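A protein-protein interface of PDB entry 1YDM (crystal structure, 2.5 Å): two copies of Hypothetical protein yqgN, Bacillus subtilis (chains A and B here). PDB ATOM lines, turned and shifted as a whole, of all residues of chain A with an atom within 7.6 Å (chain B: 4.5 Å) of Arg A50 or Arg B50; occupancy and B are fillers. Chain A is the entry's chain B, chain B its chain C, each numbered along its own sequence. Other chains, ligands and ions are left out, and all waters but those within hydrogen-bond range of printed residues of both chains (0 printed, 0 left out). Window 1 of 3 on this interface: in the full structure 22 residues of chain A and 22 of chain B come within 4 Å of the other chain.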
ATOM      1  N   THR A  47      18.332  32.452 -12.627  1.00  0.00           N
ATOM      2  CA  THR A  47      17.926  31.122 -12.179  1.00  0.00           C
ATOM      3  C   THR A  47      16.853  30.514 -13.058  1.00  0.00           C
ATOM      4  O   THR A  47      16.099  31.234 -13.707  1.00  0.00           O
ATOM      5  CB  THR A  47      17.361  31.170 -10.780  1.00  0.00           C
ATOM      6  OG1 THR A  47      16.286  32.116 -10.756  1.00  0.00           O
ATOM      7  CG2 THR A  47      18.430  31.573  -9.790  1.00  0.00           C
ATOM      8  N   ILE A  48      16.794  29.186 -13.075  1.00  0.00           N
ATOM      9  CA  ILE A  48      15.778  28.494 -13.851  1.00  0.00           C
ATOM     10  C   ILE A  48      14.484  28.551 -13.035  1.00  0.00           C
ATOM     11  O   ILE A  48      14.376  27.923 -11.982  1.00  0.00           O
ATOM     12  CB  ILE A  48      16.167  27.025 -14.117  1.00  0.00           C
ATOM     13  CG1 ILE A  48      17.520  26.964 -14.800  1.00  0.00           C
ATOM     14  CG2 ILE A  48      15.177  26.386 -15.045  1.00  0.00           C
ATOM     15  CD1 ILE A  48      18.677  27.109 -13.842  1.00  0.00           C
ATOM     16  N   SER A  49      13.502  29.300 -13.520  1.00  0.00           N
ATOM     17  CA  SER A  49      12.267  29.457 -12.768  1.00  0.00           C
ATOM     18  C   SER A  49      11.338  28.257 -12.798  1.00  0.00           C
ATOM     19  O   SER A  49      11.470  27.362 -13.636  1.00  0.00           O
ATOM     20  CB  SER A  49      11.510  30.702 -13.243  1.00  0.00           C
ATOM     21  OG  SER A  49      10.911  30.513 -14.511  1.00  0.00           O
ATOM     22  N   ARG A  50      10.391  28.237 -11.864  1.00  0.00           N
ATOM     23  CA  ARG A  50       9.430  27.149 -11.812  1.00  0.00           C
ATOM     24  C   ARG A  50       8.151  27.556 -11.103  1.00  0.00           C
ATOM     25  O   ARG A  50       8.111  28.537 -10.360  1.00  0.00           O
ATOM     26  CB  ARG A  50      10.044  25.918 -11.123  1.00  0.00           C
ATOM     27  CG  ARG A  50      10.245  26.048  -9.620  1.00  0.00           C
ATOM     28  CD  ARG A  50      10.932  24.808  -9.019  1.00  0.00           C
ATOM     29  NE  ARG A  50      10.759  24.735  -7.570  1.00  0.00           N
ATOM     30  CZ  ARG A  50      11.454  25.442  -6.680  1.00  0.00           C
ATOM     31  NH1 ARG A  50      12.399  26.281  -7.087  1.00  0.00           N
ATOM     32  NH2 ARG A  50      11.179  25.338  -5.376  1.00  0.00           N
ATOM     33  N   GLY A  51       7.101  26.794 -11.367  1.00  0.00           N
ATOM     34  CA  GLY A  51       5.824  27.028 -10.733  1.00  0.00           C
ATOM     35  C   GLY A  51       5.241  28.415 -10.808  1.00  0.00           C
ATOM     36  O   GLY A  51       4.953  28.926 -11.893  1.00  0.00           O
ATOM     37  N   LEU A  52       5.040  29.024  -9.646  1.00  0.00           N
ATOM     38  CA  LEU A  52       4.458  30.363  -9.604  1.00  0.00           C
ATOM     39  C   LEU A  52       5.491  31.483  -9.569  1.00  0.00           C
ATOM     40  O   LEU A  52       5.129  32.654  -9.491  1.00  0.00           O
ATOM     41  CB  LEU A  52       3.508  30.476  -8.417  1.00  0.00           C
ATOM     42  CG  LEU A  52       2.029  30.345  -8.750  1.00  0.00           C
ATOM     43  CD1 LEU A  52       1.805  29.422  -9.929  1.00  0.00           C
ATOM     44  CD2 LEU A  52       1.303  29.855  -7.512  1.00  0.00           C
ATOM     45  N   GLU A  53       6.768  31.113  -9.636  1.00  0.00           N
ATOM     46  CA  GLU A  53       7.836  32.089  -9.648  1.00  0.00           C
ATOM     47  C   GLU A  53       7.748  32.925 -10.932  1.00  0.00           C
ATOM     48  O   GLU A  53       6.886  32.671 -11.784  1.00  0.00           O
ATOM     49  CB  GLU A  53       9.187  31.375  -9.576  1.00  0.00           C
ATOM     50  CG  GLU A  53       9.525  30.776  -8.209  1.00  0.00           C
ATOM     51  CD  GLU A  53      10.616  29.723  -8.302  1.00  0.00           C
ATOM     52  OE1 GLU A  53      10.869  29.012  -7.308  1.00  0.00           O
ATOM     53  OE2 GLU A  53      11.217  29.597  -9.386  1.00  0.00           O
ATOM     54  N   ILE A  54       8.621  33.925 -11.073  1.00  0.00           N
ATOM     55  CA  ILE A  54       8.642  34.766 -12.279  1.00  0.00           C
ATOM     56  C   ILE A  54       9.398  34.035 -13.397  1.00  0.00           C
ATOM     57  O   ILE A  54      10.562  33.705 -13.253  1.00  0.00           O
ATOM     58  CB  ILE A  54       9.357  36.144 -12.027  1.00  0.00           C
ATOM     59  CG1 ILE A  54       8.467  37.095 -11.218  1.00  0.00           C
ATOM     60  CG2 ILE A  54       9.699  36.810 -13.358  1.00  0.00           C
ATOM     61  CD1 ILE A  54       7.224  37.571 -11.951  1.00  0.00           C
ATOM     62  N   PRO A  55       8.746  33.805 -14.542  1.00  0.00           N
ATOM     63  CA  PRO A  55       9.393  33.109 -15.657  1.00  0.00           C
ATOM     64  C   PRO A  55      10.700  33.752 -16.140  1.00  0.00           C
ATOM     65  O   PRO A  55      10.695  34.878 -16.607  1.00  0.00           O
ATOM     66  CB  PRO A  55       8.294  33.099 -16.721  1.00  0.00           C
ATOM     67  CG  PRO A  55       7.546  34.346 -16.465  1.00  0.00           C
ATOM     68  CD  PRO A  55       7.425  34.324 -14.949  1.00  0.00           C
ATOM     69  N   THR A  56      11.804  33.009 -16.036  1.00  0.00           N
ATOM     70  CA  THR A  56      13.140  33.473 -16.428  1.00  0.00           C
ATOM     71  C   THR A  56      13.583  33.118 -17.838  1.00  0.00           C
ATOM     72  O   THR A  56      14.543  33.696 -18.351  1.00  0.00           O
ATOM     73  CB  THR A  56      14.218  32.888 -15.515  1.00  0.00           C
ATOM     74  OG1 THR A  56      14.000  31.478 -15.391  1.00  0.00           O
ATOM     75  CG2 THR A  56      14.196  33.538 -14.147  1.00  0.00           C
ATOM     76  N   LYS A  74      23.952  26.515  -8.385  1.00  0.00           N
ATOM     77  CA  LYS A  74      24.044  25.091  -8.148  1.00  0.00           C
ATOM     78  C   LYS A  74      24.367  24.922  -6.667  1.00  0.00           C
ATOM     79  O   LYS A  74      25.251  24.162  -6.294  1.00  0.00           O
ATOM     80  CB  LYS A  74      25.149  24.489  -9.029  1.00  0.00           C
ATOM     81  CG  LYS A  74      25.119  22.955  -9.153  1.00  0.00           C
ATOM     82  CD  LYS A  74      23.834  22.432  -9.825  1.00  0.00           C
ATOM     83  CE  LYS A  74      22.648  22.411  -8.859  1.00  0.00           C
ATOM     84  NZ  LYS A  74      21.362  22.183  -9.568  1.00  0.00           N
ATOM     85  N   VAL A  96      14.264  22.047 -20.383  1.00  0.00           N
ATOM     86  CA  VAL A  96      14.716  22.289 -19.024  1.00  0.00           C
ATOM     87  C   VAL A  96      13.600  22.966 -18.231  1.00  0.00           C
ATOM     88  O   VAL A  96      13.312  22.579 -17.102  1.00  0.00           O
ATOM     89  CB  VAL A  96      15.955  23.210 -19.009  1.00  0.00           C
ATOM     90  CG1 VAL A  96      16.203  23.726 -17.595  1.00  0.00           C
ATOM     91  CG2 VAL A  96      17.183  22.455 -19.509  1.00  0.00           C
ATOM     92  N   TYR A  97      12.977  23.980 -18.830  1.00  0.00           N
ATOM     93  CA  TYR A  97      11.902  24.702 -18.170  1.00  0.00           C
ATOM     94  C   TYR A  97      10.677  23.819 -17.981  1.00  0.00           C
ATOM     95  O   TYR A  97       9.848  24.068 -17.104  1.00  0.00           O
ATOM     96  CB  TYR A  97      11.575  25.989 -18.937  1.00  0.00           C
ATOM     97  CG  TYR A  97      12.501  27.109 -18.534  1.00  0.00           C
ATOM     98  CD1 TYR A  97      12.111  28.059 -17.581  1.00  0.00           C
ATOM     99  CD2 TYR A  97      13.810  27.168 -19.018  1.00  0.00           C
ATOM    100  CE1 TYR A  97      13.002  29.034 -17.123  1.00  0.00           C
ATOM    101  CE2 TYR A  97      14.704  28.148 -18.556  1.00  0.00           C
ATOM    102  CZ  TYR A  97      14.289  29.075 -17.611  1.00  0.00           C
ATOM    103  OH  TYR A  97      15.150  30.061 -17.166  1.00  0.00           O
ATOM    104  N   ALA A  98      10.579  22.770 -18.791  1.00  0.00           N
ATOM    105  CA  ALA A  98       9.478  21.846 -18.645  1.00  0.00           C
ATOM    106  C   ALA A  98       9.783  20.861 -17.510  1.00  0.00           C
ATOM    107  O   ALA A  98       8.916  20.109 -17.113  1.00  0.00           O
ATOM    108  CB  ALA A  98       9.221  21.103 -19.957  1.00  0.00           C
ATOM    109  N   GLY A  99      10.994  20.904 -16.952  1.00  0.00           N
ATOM    110  CA  GLY A  99      11.353  19.988 -15.875  1.00  0.00           C
ATOM    111  C   GLY A  99      11.614  18.564 -16.371  1.00  0.00           C
ATOM    112  O   GLY A  99      11.577  17.611 -15.593  1.00  0.00           O
ATOM    113  N   LEU A 100      11.886  18.429 -17.671  1.00  0.00           N
ATOM    114  CA  LEU A 100      12.136  17.140 -18.302  1.00  0.00           C
ATOM    115  C   LEU A 100      13.592  17.000 -18.736  1.00  0.00           C
ATOM    116  O   LEU A 100      13.903  16.216 -19.632  1.00  0.00           O
ATOM    117  CB  LEU A 100      11.242  16.968 -19.530  1.00  0.00           C
ATOM    118  CG  LEU A 100       9.786  17.386 -19.415  1.00  0.00           C
ATOM    119  CD1 LEU A 100       9.149  17.361 -20.787  1.00  0.00           C
ATOM    120  CD2 LEU A 100       9.046  16.479 -18.444  1.00  0.00           C
ATOM    121  N   GLU A 102      17.451  18.276 -16.655  1.00  0.00           N
ATOM    122  CA  GLU A 102      18.229  19.177 -15.836  1.00  0.00           C
ATOM    123  C   GLU A 102      19.214  19.886 -16.746  1.00  0.00           C
ATOM    124  O   GLU A 102      19.753  19.289 -17.679  1.00  0.00           O
ATOM    125  CB  GLU A 102      18.960  18.409 -14.737  1.00  0.00           C
ATOM    126  CG  GLU A 102      18.209  18.446 -13.409  1.00  0.00           C
ATOM    127  CD  GLU A 102      18.913  17.692 -12.306  1.00  0.00           C
ATOM    128  OE1 GLU A 102      20.143  17.878 -12.140  1.00  0.00           O
ATOM    129  OE2 GLU A 102      18.234  16.918 -11.594  1.00  0.00           O
ATOM    130  N   PHE A 135      13.247  32.046  -0.335  1.00  0.00           N
ATOM    131  CA  PHE A 135      12.432  30.843  -0.457  1.00  0.00           C
ATOM    132  C   PHE A 135      12.605  29.912   0.738  1.00  0.00           C
ATOM    133  O   PHE A 135      11.819  28.982   0.932  1.00  0.00           O
ATOM    134  CB  PHE A 135      12.769  30.098  -1.756  1.00  0.00           C
ATOM    135  CG  PHE A 135      12.516  30.906  -2.991  1.00  0.00           C
ATOM    136  CD1 PHE A 135      13.483  31.777  -3.472  1.00  0.00           C
ATOM    137  CD2 PHE A 135      11.289  30.827  -3.647  1.00  0.00           C
ATOM    138  CE1 PHE A 135      13.241  32.559  -4.583  1.00  0.00           C
ATOM    139  CE2 PHE A 135      11.032  31.604  -4.760  1.00  0.00           C
ATOM    140  CZ  PHE A 135      12.016  32.475  -5.229  1.00  0.00           C
ATOM    141  N   ILE B  48       9.476  16.087  -5.220  1.00  0.00           N
ATOM    142  CA  ILE B  48       8.570  17.226  -5.370  1.00  0.00           C
ATOM    143  C   ILE B  48       8.516  17.510  -6.859  1.00  0.00           C
ATOM    144  O   ILE B  48       9.495  17.981  -7.436  1.00  0.00           O
ATOM    145  CB  ILE B  48       9.094  18.506  -4.676  1.00  0.00           C
ATOM    146  CG1 ILE B  48       9.282  18.263  -3.176  1.00  0.00           C
ATOM    147  CG2 ILE B  48       8.097  19.621  -4.882  1.00  0.00           C
ATOM    148  CD1 ILE B  48       7.980  17.909  -2.466  1.00  0.00           C
ATOM    149  N   SER B  49       7.377  17.236  -7.481  1.00  0.00           N
ATOM    150  CA  SER B  49       7.233  17.454  -8.918  1.00  0.00           C
ATOM    151  C   SER B  49       7.286  18.902  -9.375  1.00  0.00           C
ATOM    152  O   SER B  49       7.121  19.829  -8.581  1.00  0.00           O
ATOM    153  CB  SER B  49       5.939  16.831  -9.412  1.00  0.00           C
ATOM    154  OG  SER B  49       4.906  17.062  -8.484  1.00  0.00           O
ATOM    155  N   ARG B  50       7.527  19.092 -10.668  1.00  0.00           N
ATOM    156  CA  ARG B  50       7.588  20.436 -11.236  1.00  0.00           C
ATOM    157  C   ARG B  50       7.338  20.408 -12.743  1.00  0.00           C
ATOM    158  O   ARG B  50       7.517  19.376 -13.388  1.00  0.00           O
ATOM    159  CB  ARG B  50       8.946  21.091 -10.954  1.00  0.00           C
ATOM    160  CG  ARG B  50      10.031  20.723 -11.949  1.00  0.00           C
ATOM    161  CD  ARG B  50      11.316  21.500 -11.682  1.00  0.00           C
ATOM    162  NE  ARG B  50      12.255  20.762 -10.852  1.00  0.00           N
ATOM    163  CZ  ARG B  50      13.219  21.325 -10.124  1.00  0.00           C
ATOM    164  NH1 ARG B  50      13.383  22.647 -10.112  1.00  0.00           N
ATOM    165  NH2 ARG B  50      14.025  20.565  -9.389  1.00  0.00           N
ATOM    166  N   GLY B  51       6.905  21.545 -13.284  1.00  0.00           N
ATOM    167  CA  GLY B  51       6.642  21.660 -14.702  1.00  0.00           C
ATOM    168  C   GLY B  51       5.667  20.640 -15.246  1.00  0.00           C
ATOM    169  O   GLY B  51       4.535  20.526 -14.765  1.00  0.00           O
ATOM    170  N   LEU B  52       6.112  19.897 -16.259  1.00  0.00           N
ATOM    171  CA  LEU B  52       5.297  18.860 -16.895  1.00  0.00           C
ATOM    172  C   LEU B  52       5.529  17.496 -16.238  1.00  0.00           C
ATOM    173  O   LEU B  52       4.912  16.498 -16.635  1.00  0.00           O
ATOM    174  CB  LEU B  52       5.628  18.779 -18.385  1.00  0.00           C
ATOM    175  CG  LEU B  52       5.298  20.050 -19.178  1.00  0.00           C
ATOM    176  CD1 LEU B  52       5.906  20.043 -20.593  1.00  0.00           C
ATOM    177  CD2 LEU B  52       3.797  20.150 -19.240  1.00  0.00           C
ATOM    178  N   GLU B  53       6.421  17.439 -15.249  1.00  0.00           N
ATOM    179  CA  GLU B  53       6.647  16.172 -14.565  1.00  0.00           C
ATOM    180  C   GLU B  53       5.341  15.741 -13.944  1.00  0.00           C
ATOM    181  O   GLU B  53       4.545  16.579 -13.511  1.00  0.00           O
ATOM    182  CB  GLU B  53       7.685  16.301 -13.459  1.00  0.00           C
ATOM    183  CG  GLU B  53       9.105  16.424 -13.937  1.00  0.00           C
ATOM    184  CD  GLU B  53       9.984  16.989 -12.868  1.00  0.00           C
ATOM    185  OE1 GLU B  53      11.053  17.536 -13.198  1.00  0.00           O
ATOM    186  OE2 GLU B  53       9.616  16.893 -11.675  1.00  0.00           O
ATOM    187  N   ALA B  98       4.532  25.192  -5.579  1.00  0.00           N
ATOM    188  CA  ALA B  98       4.317  26.382  -6.373  1.00  0.00           C
ATOM    189  C   ALA B  98       5.625  27.139  -6.571  1.00  0.00           C
ATOM    190  O   ALA B  98       5.644  28.186  -7.213  1.00  0.00           O
ATOM    191  CB  ALA B  98       3.294  27.276  -5.690  1.00  0.00           C
ATOM    192  N   GLY B  99       6.707  26.610  -6.014  1.00  0.00           N
ATOM    193  CA  GLY B  99       8.006  27.240  -6.163  1.00  0.00           C
ATOM    194  C   GLY B  99       8.212  28.434  -5.252  1.00  0.00           C
ATOM    195  O   GLY B  99       9.113  29.255  -5.469  1.00  0.00           O
ATOM    196  N   GLU B 102      10.986  26.166  -0.255  1.00  0.00           N
ATOM    197  CA  GLU B 102      11.776  24.957  -0.349  1.00  0.00           C
ATOM    198  C   GLU B 102      11.530  24.123   0.899  1.00  0.00           C
ATOM    199  O   GLU B 102      11.605  24.636   2.016  1.00  0.00           O
ATOM    200  CB  GLU B 102      13.262  25.289  -0.479  1.00  0.00           C
ATOM    201  CG  GLU B 102      13.648  25.881  -1.830  1.00  0.00           C
ATOM    202  CD  GLU B 102      15.121  26.233  -1.904  1.00  0.00           C
ATOM    203  OE1 GLU B 102      15.561  26.758  -2.951  1.00  0.00           O
ATOM    204  OE2 GLU B 102      15.843  25.985  -0.911  1.00  0.00           O
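N of Leu A52 is in hydrogen-bond range of O of Ala B98, at 2.6 Å. The backbone carbonyl oxygen (O) of Gly B99 sits close to the side-chain carboxylate (OE1) of Glu A53, 2.6 Å away. The backbone carbonyl oxygen of Ala A98 lies within hydrogen-bond range of the backbone NH of Leu B52. The backbone carbonyl oxygen (O) of Gly A99 sits close to the side-chain carboxylate (OE1) of Glu B53. The backbone carbonyl oxygen (O) of Phe A135 is in hydrogen-bond range of the backbone NH (N) of Glu B102, 3.2 Å away.
NH1 of Arg A50 is in salt-bridge range of OE1 of Glu A53 (3.1 Å). N of Arg B50 sits at hydrogen-bond distance from OE2 of Glu B53.
Among the printed residues, pairs that only touch across the chains: Phe A135 with Gly B99, Arg A50 with Arg B50, Gly A51 with Ala B98, Ala A98 with Gly B51, Arg A50 with Gly B99 and Glu A53 with Ala B98.
Of the printed residues of chain B, Leu A52 touches Ala B98. Printed residues of chain B within 4 Å of Ala A98: Gly B51 and Leu B52. Of the printed residues of chain B, Gly A99 touches Glu B53 (2.5 Å). Of chain A, only Arg A50 comes within 4 Å of Arg B50. Of the printed residues of chain A, Gly B51 touches Ala A98 (3.7 Å). Printed residues of chain A within 4 Å of Gly B99: Arg A50 (3.8 Å), Glu A53 (2.6 Å) and Phe A135 (3.1 Å). Of the printed residues of chain A, Glu B102 touches Phe A135 (3.2 Å). The nearest residue of chain A that does not touch Arg B50 is Ala A98 (4.05 Å).
Of the 18 printed residues of chain A, 7 touch a printed residue of chain B. Printed residues of chain A that touch a printed residue of chain B: Arg A50, Gly A51, Leu A52, Glu A53, Ala A98, Gly A99 and Phe A135. Printed residues of chain B that touch a printed residue of chain A: Arg B50, Gly B51, Leu B52, Glu B53, Ala B98, Gly B99 and Glu B102. Among the printed residues, 11 pairs touch across the chains. Among the printed residues, no Asp or Glu carboxylate lies within 4 Å of a Lys or Arg side-chain nitrogen of the other chain.
Gly A51 touches Ala B98, and with the chains exchanged Ala A98 touches Gly B51. Leu A52 touches Ala B98, and with the chains exchanged Ala A98 touches Leu B52. Glu A53 touches Ala B98, but with the chains exchanged Ala A98 does not touch Glu B53 (4.1 Å). Glu A53 touches Gly B99, and with the chains exchanged Gly A99 touches Glu B53.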
